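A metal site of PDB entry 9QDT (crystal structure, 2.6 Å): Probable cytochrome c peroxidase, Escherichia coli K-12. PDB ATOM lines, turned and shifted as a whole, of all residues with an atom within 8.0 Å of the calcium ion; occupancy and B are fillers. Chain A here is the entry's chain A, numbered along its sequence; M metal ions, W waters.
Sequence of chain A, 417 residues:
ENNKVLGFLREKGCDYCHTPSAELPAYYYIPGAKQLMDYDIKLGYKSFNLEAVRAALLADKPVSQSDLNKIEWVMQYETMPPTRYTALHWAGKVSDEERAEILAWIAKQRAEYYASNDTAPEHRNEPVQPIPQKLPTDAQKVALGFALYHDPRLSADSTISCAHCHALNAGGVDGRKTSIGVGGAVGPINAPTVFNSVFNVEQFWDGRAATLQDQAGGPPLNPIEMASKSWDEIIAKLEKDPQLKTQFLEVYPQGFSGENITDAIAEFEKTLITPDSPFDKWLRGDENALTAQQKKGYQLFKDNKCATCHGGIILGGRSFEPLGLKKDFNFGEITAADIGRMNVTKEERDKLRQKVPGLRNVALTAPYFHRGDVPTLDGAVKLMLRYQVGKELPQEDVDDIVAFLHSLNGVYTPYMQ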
ATOM      1  N   VAL A 173      22.723 -22.357 -34.511  1.00  0.00           N
ATOM      2  CA  VAL A 173      22.373 -23.255 -33.427  1.00  0.00           C
ATOM      3  C   VAL A 173      22.647 -24.703 -33.859  1.00  0.00           C
ATOM      4  O   VAL A 173      22.814 -24.963 -35.054  1.00  0.00           O
ATOM      5  CB  VAL A 173      20.899 -22.822 -33.324  1.00  0.00           C
ATOM      6  CG1 VAL A 173      19.928 -23.968 -33.429  1.00  0.00           C
ATOM      7  CG2 VAL A 173      20.635 -21.893 -32.140  1.00  0.00           C
ATOM      8  N   ASP A 174      22.713 -25.646 -32.894  1.00  0.00           N
ATOM      9  CA  ASP A 174      23.054 -27.028 -33.204  1.00  0.00           C
ATOM     10  C   ASP A 174      21.816 -27.902 -33.418  1.00  0.00           C
ATOM     11  O   ASP A 174      21.949 -29.052 -33.866  1.00  0.00           O
ATOM     12  CB  ASP A 174      23.940 -27.621 -32.133  1.00  0.00           C
ATOM     13  CG  ASP A 174      23.431 -27.520 -30.704  1.00  0.00           C
ATOM     14  OD1 ASP A 174      22.210 -27.181 -30.515  1.00  0.00           O
ATOM     15  OD2 ASP A 174      24.265 -27.759 -29.785  1.00  0.00           O
ATOM     16  N   GLY A 175      20.632 -27.386 -33.055  1.00  0.00           N
ATOM     17  CA  GLY A 175      19.372 -28.081 -33.238  1.00  0.00           C
ATOM     18  C   GLY A 175      19.168 -29.237 -32.250  1.00  0.00           C
ATOM     19  O   GLY A 175      18.246 -30.028 -32.375  1.00  0.00           O
ATOM     20  N   ARG A 176      20.063 -29.329 -31.269  1.00  0.00           N
ATOM     21  CA  ARG A 176      19.966 -30.305 -30.209  1.00  0.00           C
ATOM     22  C   ARG A 176      19.254 -29.696 -28.995  1.00  0.00           C
ATOM     23  O   ARG A 176      19.182 -28.475 -28.831  1.00  0.00           O
ATOM     24  CB  ARG A 176      21.368 -30.703 -29.760  1.00  0.00           C
ATOM     25  CG  ARG A 176      22.361 -31.100 -30.829  1.00  0.00           C
ATOM     26  CD  ARG A 176      23.695 -31.534 -30.205  1.00  0.00           C
ATOM     27  NE  ARG A 176      24.710 -31.824 -31.232  1.00  0.00           N
ATOM     28  CZ  ARG A 176      24.892 -33.013 -31.749  1.00  0.00           C
ATOM     29  NH1 ARG A 176      24.216 -34.055 -31.296  1.00  0.00           N
ATOM     30  NH2 ARG A 176      25.766 -33.155 -32.709  1.00  0.00           N
ATOM     31  N   LYS A 177      18.760 -30.595 -28.132  1.00  0.00           N
ATOM     32  CA  LYS A 177      18.102 -30.248 -26.889  1.00  0.00           C
ATOM     33  C   LYS A 177      19.050 -29.422 -26.013  1.00  0.00           C
ATOM     34  O   LYS A 177      18.701 -28.351 -25.545  1.00  0.00           O
ATOM     35  CB  LYS A 177      17.713 -31.587 -26.267  1.00  0.00           C
ATOM     36  CG  LYS A 177      16.878 -31.427 -25.051  1.00  0.00           C
ATOM     37  CD  LYS A 177      16.567 -32.716 -24.317  1.00  0.00           C
ATOM     38  CE  LYS A 177      15.587 -32.379 -23.247  1.00  0.00           C
ATOM     39  NZ  LYS A 177      15.586 -33.379 -22.182  1.00  0.00           N
ATOM     40  N   ASN A 190      19.851 -25.247 -23.582  1.00  0.00           N
ATOM     41  CA  ASN A 190      19.736 -25.135 -25.026  1.00  0.00           C
ATOM     42  C   ASN A 190      20.604 -23.980 -25.489  1.00  0.00           C
ATOM     43  O   ASN A 190      20.560 -22.919 -24.896  1.00  0.00           O
ATOM     44  CB  ASN A 190      18.275 -24.888 -25.433  1.00  0.00           C
ATOM     45  CG  ASN A 190      18.021 -24.928 -26.922  1.00  0.00           C
ATOM     46  OD1 ASN A 190      17.724 -23.899 -27.572  1.00  0.00           O
ATOM     47  ND2 ASN A 190      18.086 -26.110 -27.506  1.00  0.00           N
ATOM     48  N   ALA A 191      21.331 -24.191 -26.577  1.00  0.00           N
ATOM     49  CA  ALA A 191      22.236 -23.183 -27.112  1.00  0.00           C
ATOM     50  C   ALA A 191      21.407 -22.210 -27.915  1.00  0.00           C
ATOM     51  O   ALA A 191      20.732 -22.596 -28.849  1.00  0.00           O
ATOM     52  CB  ALA A 191      23.290 -23.832 -27.983  1.00  0.00           C
ATOM     53  N   PRO A 192      21.455 -20.903 -27.584  1.00  0.00           N
ATOM     54  CA  PRO A 192      20.723 -19.916 -28.358  1.00  0.00           C
ATOM     55  C   PRO A 192      21.505 -19.548 -29.606  1.00  0.00           C
ATOM     56  O   PRO A 192      22.683 -19.880 -29.721  1.00  0.00           O
ATOM     57  CB  PRO A 192      20.609 -18.751 -27.388  1.00  0.00           C
ATOM     58  CG  PRO A 192      21.874 -18.856 -26.562  1.00  0.00           C
ATOM     59  CD  PRO A 192      22.157 -20.340 -26.435  1.00  0.00           C
ATOM     60  N   THR A 193      20.811 -18.856 -30.517  1.00  0.00           N
ATOM     61  CA  THR A 193      21.377 -18.377 -31.758  1.00  0.00           C
ATOM     62  C   THR A 193      22.380 -17.251 -31.516  1.00  0.00           C
ATOM     63  O   THR A 193      22.210 -16.383 -30.662  1.00  0.00           O
ATOM     64  CB  THR A 193      20.234 -17.947 -32.681  1.00  0.00           C
ATOM     65  OG1 THR A 193      20.880 -17.705 -33.929  1.00  0.00           O
ATOM     66  CG2 THR A 193      19.505 -16.728 -32.138  1.00  0.00           C
ATOM     67  N   TRP A 205      21.666 -17.270 -20.930  1.00  0.00           N
ATOM     68  CA  TRP A 205      20.304 -17.274 -20.416  1.00  0.00           C
ATOM     69  C   TRP A 205      20.253 -16.535 -19.079  1.00  0.00           C
ATOM     70  O   TRP A 205      19.296 -15.807 -18.829  1.00  0.00           O
ATOM     71  CB  TRP A 205      19.798 -18.716 -20.274  1.00  0.00           C
ATOM     72  CG  TRP A 205      19.377 -19.387 -21.548  1.00  0.00           C
ATOM     73  CD1 TRP A 205      20.109 -20.254 -22.320  1.00  0.00           C
ATOM     74  CD2 TRP A 205      18.085 -19.299 -22.173  1.00  0.00           C
ATOM     75  NE1 TRP A 205      19.364 -20.685 -23.382  1.00  0.00           N
ATOM     76  CE2 TRP A 205      18.117 -20.114 -23.322  1.00  0.00           C
ATOM     77  CE3 TRP A 205      16.908 -18.592 -21.876  1.00  0.00           C
ATOM     78  CZ2 TRP A 205      17.021 -20.262 -24.163  1.00  0.00           C
ATOM     79  CZ3 TRP A 205      15.815 -18.753 -22.696  1.00  0.00           C
ATOM     80  CH2 TRP A 205      15.872 -19.574 -23.824  1.00  0.00           C
ATOM     81  N   PRO A 357      14.095 -14.614 -24.710  1.00  0.00           N
ATOM     82  CA  PRO A 357      14.707 -14.860 -26.016  1.00  0.00           C
ATOM     83  C   PRO A 357      14.137 -13.921 -27.059  1.00  0.00           C
ATOM     84  O   PRO A 357      12.918 -13.726 -27.108  1.00  0.00           O
ATOM     85  CB  PRO A 357      14.348 -16.316 -26.337  1.00  0.00           C
ATOM     86  CG  PRO A 357      13.718 -16.848 -25.086  1.00  0.00           C
ATOM     87  CD  PRO A 357      13.188 -15.690 -24.289  1.00  0.00           C
ATOM     88  N   VAL A 362      13.221 -17.466 -34.925  1.00  0.00           N
ATOM     89  CA  VAL A 362      12.841 -18.538 -34.011  1.00  0.00           C
ATOM     90  C   VAL A 362      12.352 -19.755 -34.799  1.00  0.00           C
ATOM     91  O   VAL A 362      12.459 -20.888 -34.331  1.00  0.00           O
ATOM     92  CB  VAL A 362      11.776 -18.092 -32.997  1.00  0.00           C
ATOM     93  CG1 VAL A 362      10.463 -17.740 -33.670  1.00  0.00           C
ATOM     94  CG2 VAL A 362      11.568 -19.166 -31.929  1.00  0.00           C
ATOM     95  N   LEU A 364      13.757 -21.078 -37.047  1.00  0.00           N
ATOM     96  CA  LEU A 364      14.922 -21.822 -37.476  1.00  0.00           C
ATOM     97  C   LEU A 364      15.728 -22.381 -36.296  1.00  0.00           C
ATOM     98  O   LEU A 364      16.766 -22.989 -36.551  1.00  0.00           O
ATOM     99  CB  LEU A 364      15.866 -20.923 -38.266  1.00  0.00           C
ATOM    100  CG  LEU A 364      15.294 -20.201 -39.490  1.00  0.00           C
ATOM    101  CD1 LEU A 364      16.431 -19.368 -40.077  1.00  0.00           C
ATOM    102  CD2 LEU A 364      14.686 -21.179 -40.496  1.00  0.00           C
ATOM    103  N   THR A 365      15.316 -22.109 -35.045  1.00  0.00           N
ATOM    104  CA  THR A 365      16.136 -22.460 -33.889  1.00  0.00           C
ATOM    105  C   THR A 365      15.449 -23.490 -32.964  1.00  0.00           C
ATOM    106  O   THR A 365      15.798 -23.566 -31.787  1.00  0.00           O
ATOM    107  CB  THR A 365      16.475 -21.151 -33.183  1.00  0.00           C
ATOM    108  OG1 THR A 365      15.283 -20.492 -32.735  1.00  0.00           O
ATOM    109  CG2 THR A 365      17.155 -20.202 -34.147  1.00  0.00           C
ATOM    110  N   ALA A 366      14.514 -24.300 -33.494  1.00  0.00           N
ATOM    111  CA  ALA A 366      14.055 -25.485 -32.768  1.00  0.00           C
ATOM    112  C   ALA A 366      15.212 -26.330 -32.226  1.00  0.00           C
ATOM    113  O   ALA A 366      16.327 -26.297 -32.727  1.00  0.00           O
ATOM    114  CB  ALA A 366      13.178 -26.329 -33.660  1.00  0.00           C
ATOM    115  N   PRO A 367      15.038 -27.083 -31.116  1.00  0.00           N
ATOM    116  CA  PRO A 367      13.849 -27.000 -30.260  1.00  0.00           C
ATOM    117  C   PRO A 367      13.885 -25.784 -29.328  1.00  0.00           C
ATOM    118  O   PRO A 367      14.913 -25.089 -29.271  1.00  0.00           O
ATOM    119  CB  PRO A 367      13.935 -28.312 -29.475  1.00  0.00           C
ATOM    120  CG  PRO A 367      15.421 -28.558 -29.320  1.00  0.00           C
ATOM    121  CD  PRO A 367      16.021 -28.057 -30.629  1.00  0.00           C
ATOM    122  N   TYR A 368      12.776 -25.577 -28.580  1.00  0.00           N
ATOM    123  CA  TYR A 368      12.537 -24.315 -27.885  1.00  0.00           C
ATOM    124  C   TYR A 368      12.602 -24.443 -26.367  1.00  0.00           C
ATOM    125  O   TYR A 368      12.636 -25.546 -25.823  1.00  0.00           O
ATOM    126  CB  TYR A 368      11.173 -23.806 -28.363  1.00  0.00           C
ATOM    127  CG  TYR A 368      11.172 -23.641 -29.862  1.00  0.00           C
ATOM    128  CD1 TYR A 368      11.945 -22.656 -30.445  1.00  0.00           C
ATOM    129  CD2 TYR A 368      10.445 -24.481 -30.690  1.00  0.00           C
ATOM    130  CE1 TYR A 368      12.016 -22.519 -31.813  1.00  0.00           C
ATOM    131  CE2 TYR A 368      10.502 -24.358 -32.068  1.00  0.00           C
ATOM    132  CZ  TYR A 368      11.300 -23.378 -32.630  1.00  0.00           C
ATOM    133  OH  TYR A 368      11.339 -23.201 -33.978  1.00  0.00           O
ATOM    134  N   PHE A 369      12.577 -23.269 -25.708  1.00  0.00           N
ATOM    135  CA  PHE A 369      12.709 -23.080 -24.270  1.00  0.00           C
ATOM    136  C   PHE A 369      14.124 -23.440 -23.838  1.00  0.00           C
ATOM    137  O   PHE A 369      14.898 -24.046 -24.581  1.00  0.00           O
ATOM    138  CB  PHE A 369      11.628 -23.803 -23.449  1.00  0.00           C
ATOM    139  CG  PHE A 369      10.223 -23.220 -23.510  1.00  0.00           C
ATOM    140  CD1 PHE A 369       9.784 -22.449 -24.573  1.00  0.00           C
ATOM    141  CD2 PHE A 369       9.347 -23.397 -22.461  1.00  0.00           C
ATOM    142  CE1 PHE A 369       8.506 -21.907 -24.594  1.00  0.00           C
ATOM    143  CE2 PHE A 369       8.061 -22.856 -22.487  1.00  0.00           C
ATOM    144  CZ  PHE A 369       7.646 -22.119 -23.559  1.00  0.00           C
ATOM    145  N   HIS A 370      14.503 -22.991 -22.651  1.00  0.00           N
ATOM    146  CA  HIS A 370      15.879 -23.142 -22.211  1.00  0.00           C
ATOM    147  C   HIS A 370      16.230 -24.617 -22.001  1.00  0.00           C
ATOM    148  O   HIS A 370      17.408 -24.989 -22.059  1.00  0.00           O
ATOM    149  CB  HIS A 370      16.158 -22.252 -21.001  1.00  0.00           C
ATOM    150  CG  HIS A 370      15.675 -22.770 -19.685  1.00  0.00           C
ATOM    151  ND1 HIS A 370      14.624 -22.199 -18.997  1.00  0.00           N
ATOM    152  CD2 HIS A 370      16.138 -23.763 -18.930  1.00  0.00           C
ATOM    153  CE1 HIS A 370      14.457 -22.859 -17.855  1.00  0.00           C
ATOM    154  NE2 HIS A 370      15.364 -23.826 -17.796  1.00  0.00           N
ATOM    155  N   ARG A 371      15.231 -25.456 -21.740  1.00  0.00           N
ATOM    156  CA  ARG A 371      15.408 -26.885 -21.488  1.00  0.00           C
ATOM    157  C   ARG A 371      15.556 -27.640 -22.804  1.00  0.00           C
ATOM    158  O   ARG A 371      15.959 -28.804 -22.811  1.00  0.00           O
ATOM    159  CB  ARG A 371      14.218 -27.422 -20.654  1.00  0.00           C
ATOM    160  CG  ARG A 371      14.610 -27.587 -19.204  1.00  0.00           C
ATOM    161  CD  ARG A 371      13.709 -27.127 -18.094  1.00  0.00           C
ATOM    162  NE  ARG A 371      12.798 -28.139 -17.609  1.00  0.00           N
ATOM    163  CZ  ARG A 371      12.616 -28.646 -16.396  1.00  0.00           C
ATOM    164  NH1 ARG A 371      13.249 -28.287 -15.294  1.00  0.00           N
ATOM    165  NH2 ARG A 371      11.691 -29.554 -16.303  1.00  0.00           N
ATOM    166  N   GLY A 372      15.141 -27.025 -23.913  1.00  0.00           N
ATOM    167  CA  GLY A 372      15.297 -27.586 -25.237  1.00  0.00           C
ATOM    168  C   GLY A 372      14.295 -28.700 -25.486  1.00  0.00           C
ATOM    169  O   GLY A 372      14.505 -29.539 -26.382  1.00  0.00           O
ATOM    170  N   ASP A 373      13.208 -28.677 -24.725  1.00  0.00           N
ATOM    171  CA  ASP A 373      12.286 -29.822 -24.666  1.00  0.00           C
ATOM    172  C   ASP A 373      10.964 -29.502 -25.353  1.00  0.00           C
ATOM    173  O   ASP A 373      10.029 -30.292 -25.288  1.00  0.00           O
ATOM    174  CB  ASP A 373      12.045 -30.263 -23.230  1.00  0.00           C
ATOM    175  CG  ASP A 373      11.418 -29.239 -22.290  1.00  0.00           C
ATOM    176  OD1 ASP A 373      11.345 -28.014 -22.668  1.00  0.00           O
ATOM    177  OD2 ASP A 373      11.001 -29.667 -21.169  1.00  0.00           O
ATOM    178  N   VAL A 374      10.847 -28.326 -25.986  1.00  0.00           N
ATOM    179  CA  VAL A 374       9.592 -27.969 -26.639  1.00  0.00           C
ATOM    180  C   VAL A 374       9.834 -28.027 -28.130  1.00  0.00           C
ATOM    181  O   VAL A 374      10.486 -27.157 -28.681  1.00  0.00           O
ATOM    182  CB  VAL A 374       9.083 -26.592 -26.217  1.00  0.00           C
ATOM    183  CG1 VAL A 374       7.843 -26.169 -27.006  1.00  0.00           C
ATOM    184  CG2 VAL A 374       8.840 -26.547 -24.720  1.00  0.00           C
HETATM  185 CA    CA M   1      16.307 -23.175 -29.352  1.00  0.00          CA
HETATM  186  O   HOH W   1      17.542 -25.025 -30.444  1.00  0.00           O
HETATM  187  O   HOH W   2      15.336 -22.598 -27.226  1.00  0.00           O
HETATM  188  O   HOH W   3      18.350 -22.098 -30.007  1.00  0.00           O
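The side-chain amide nitrogen (ND2) of Asn 190 lies within hydrogen-bond range of the backbone carbonyl oxygen (O) of Lys 177 (3.0 Å).
ND2 of Asn 190 lies within hydrogen-bond range of O of Arg 176 (2.9 Å).
The backbone NH (N) of Asn 190 sits at hydrogen-bond distance from the backbone carbonyl oxygen (O) of His 370 (2.9 Å).
NE1 of Trp 205 is in hydrogen-bond range of O of Asn 190 (3.0 Å).
OG1 of Thr 365 is in hydrogen-bond range of O of Val 362 (3.3 Å).
Of the 23 residues printed, 3 come within 4 Å of the calcium ion.
Water W1 bridges O of Ala 366 (2.9 Å) and ND2 of Asn 190 (3.2 Å).
The calcium ion is bound by O of Pro 367 (2.4 Å), OD1 of Asn 190 (2.4 Å), water W3 (2.4 Å), water W2 (2.4 Å), water W1 (2.5 Å) and O of Thr 365 (2.5 Å).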
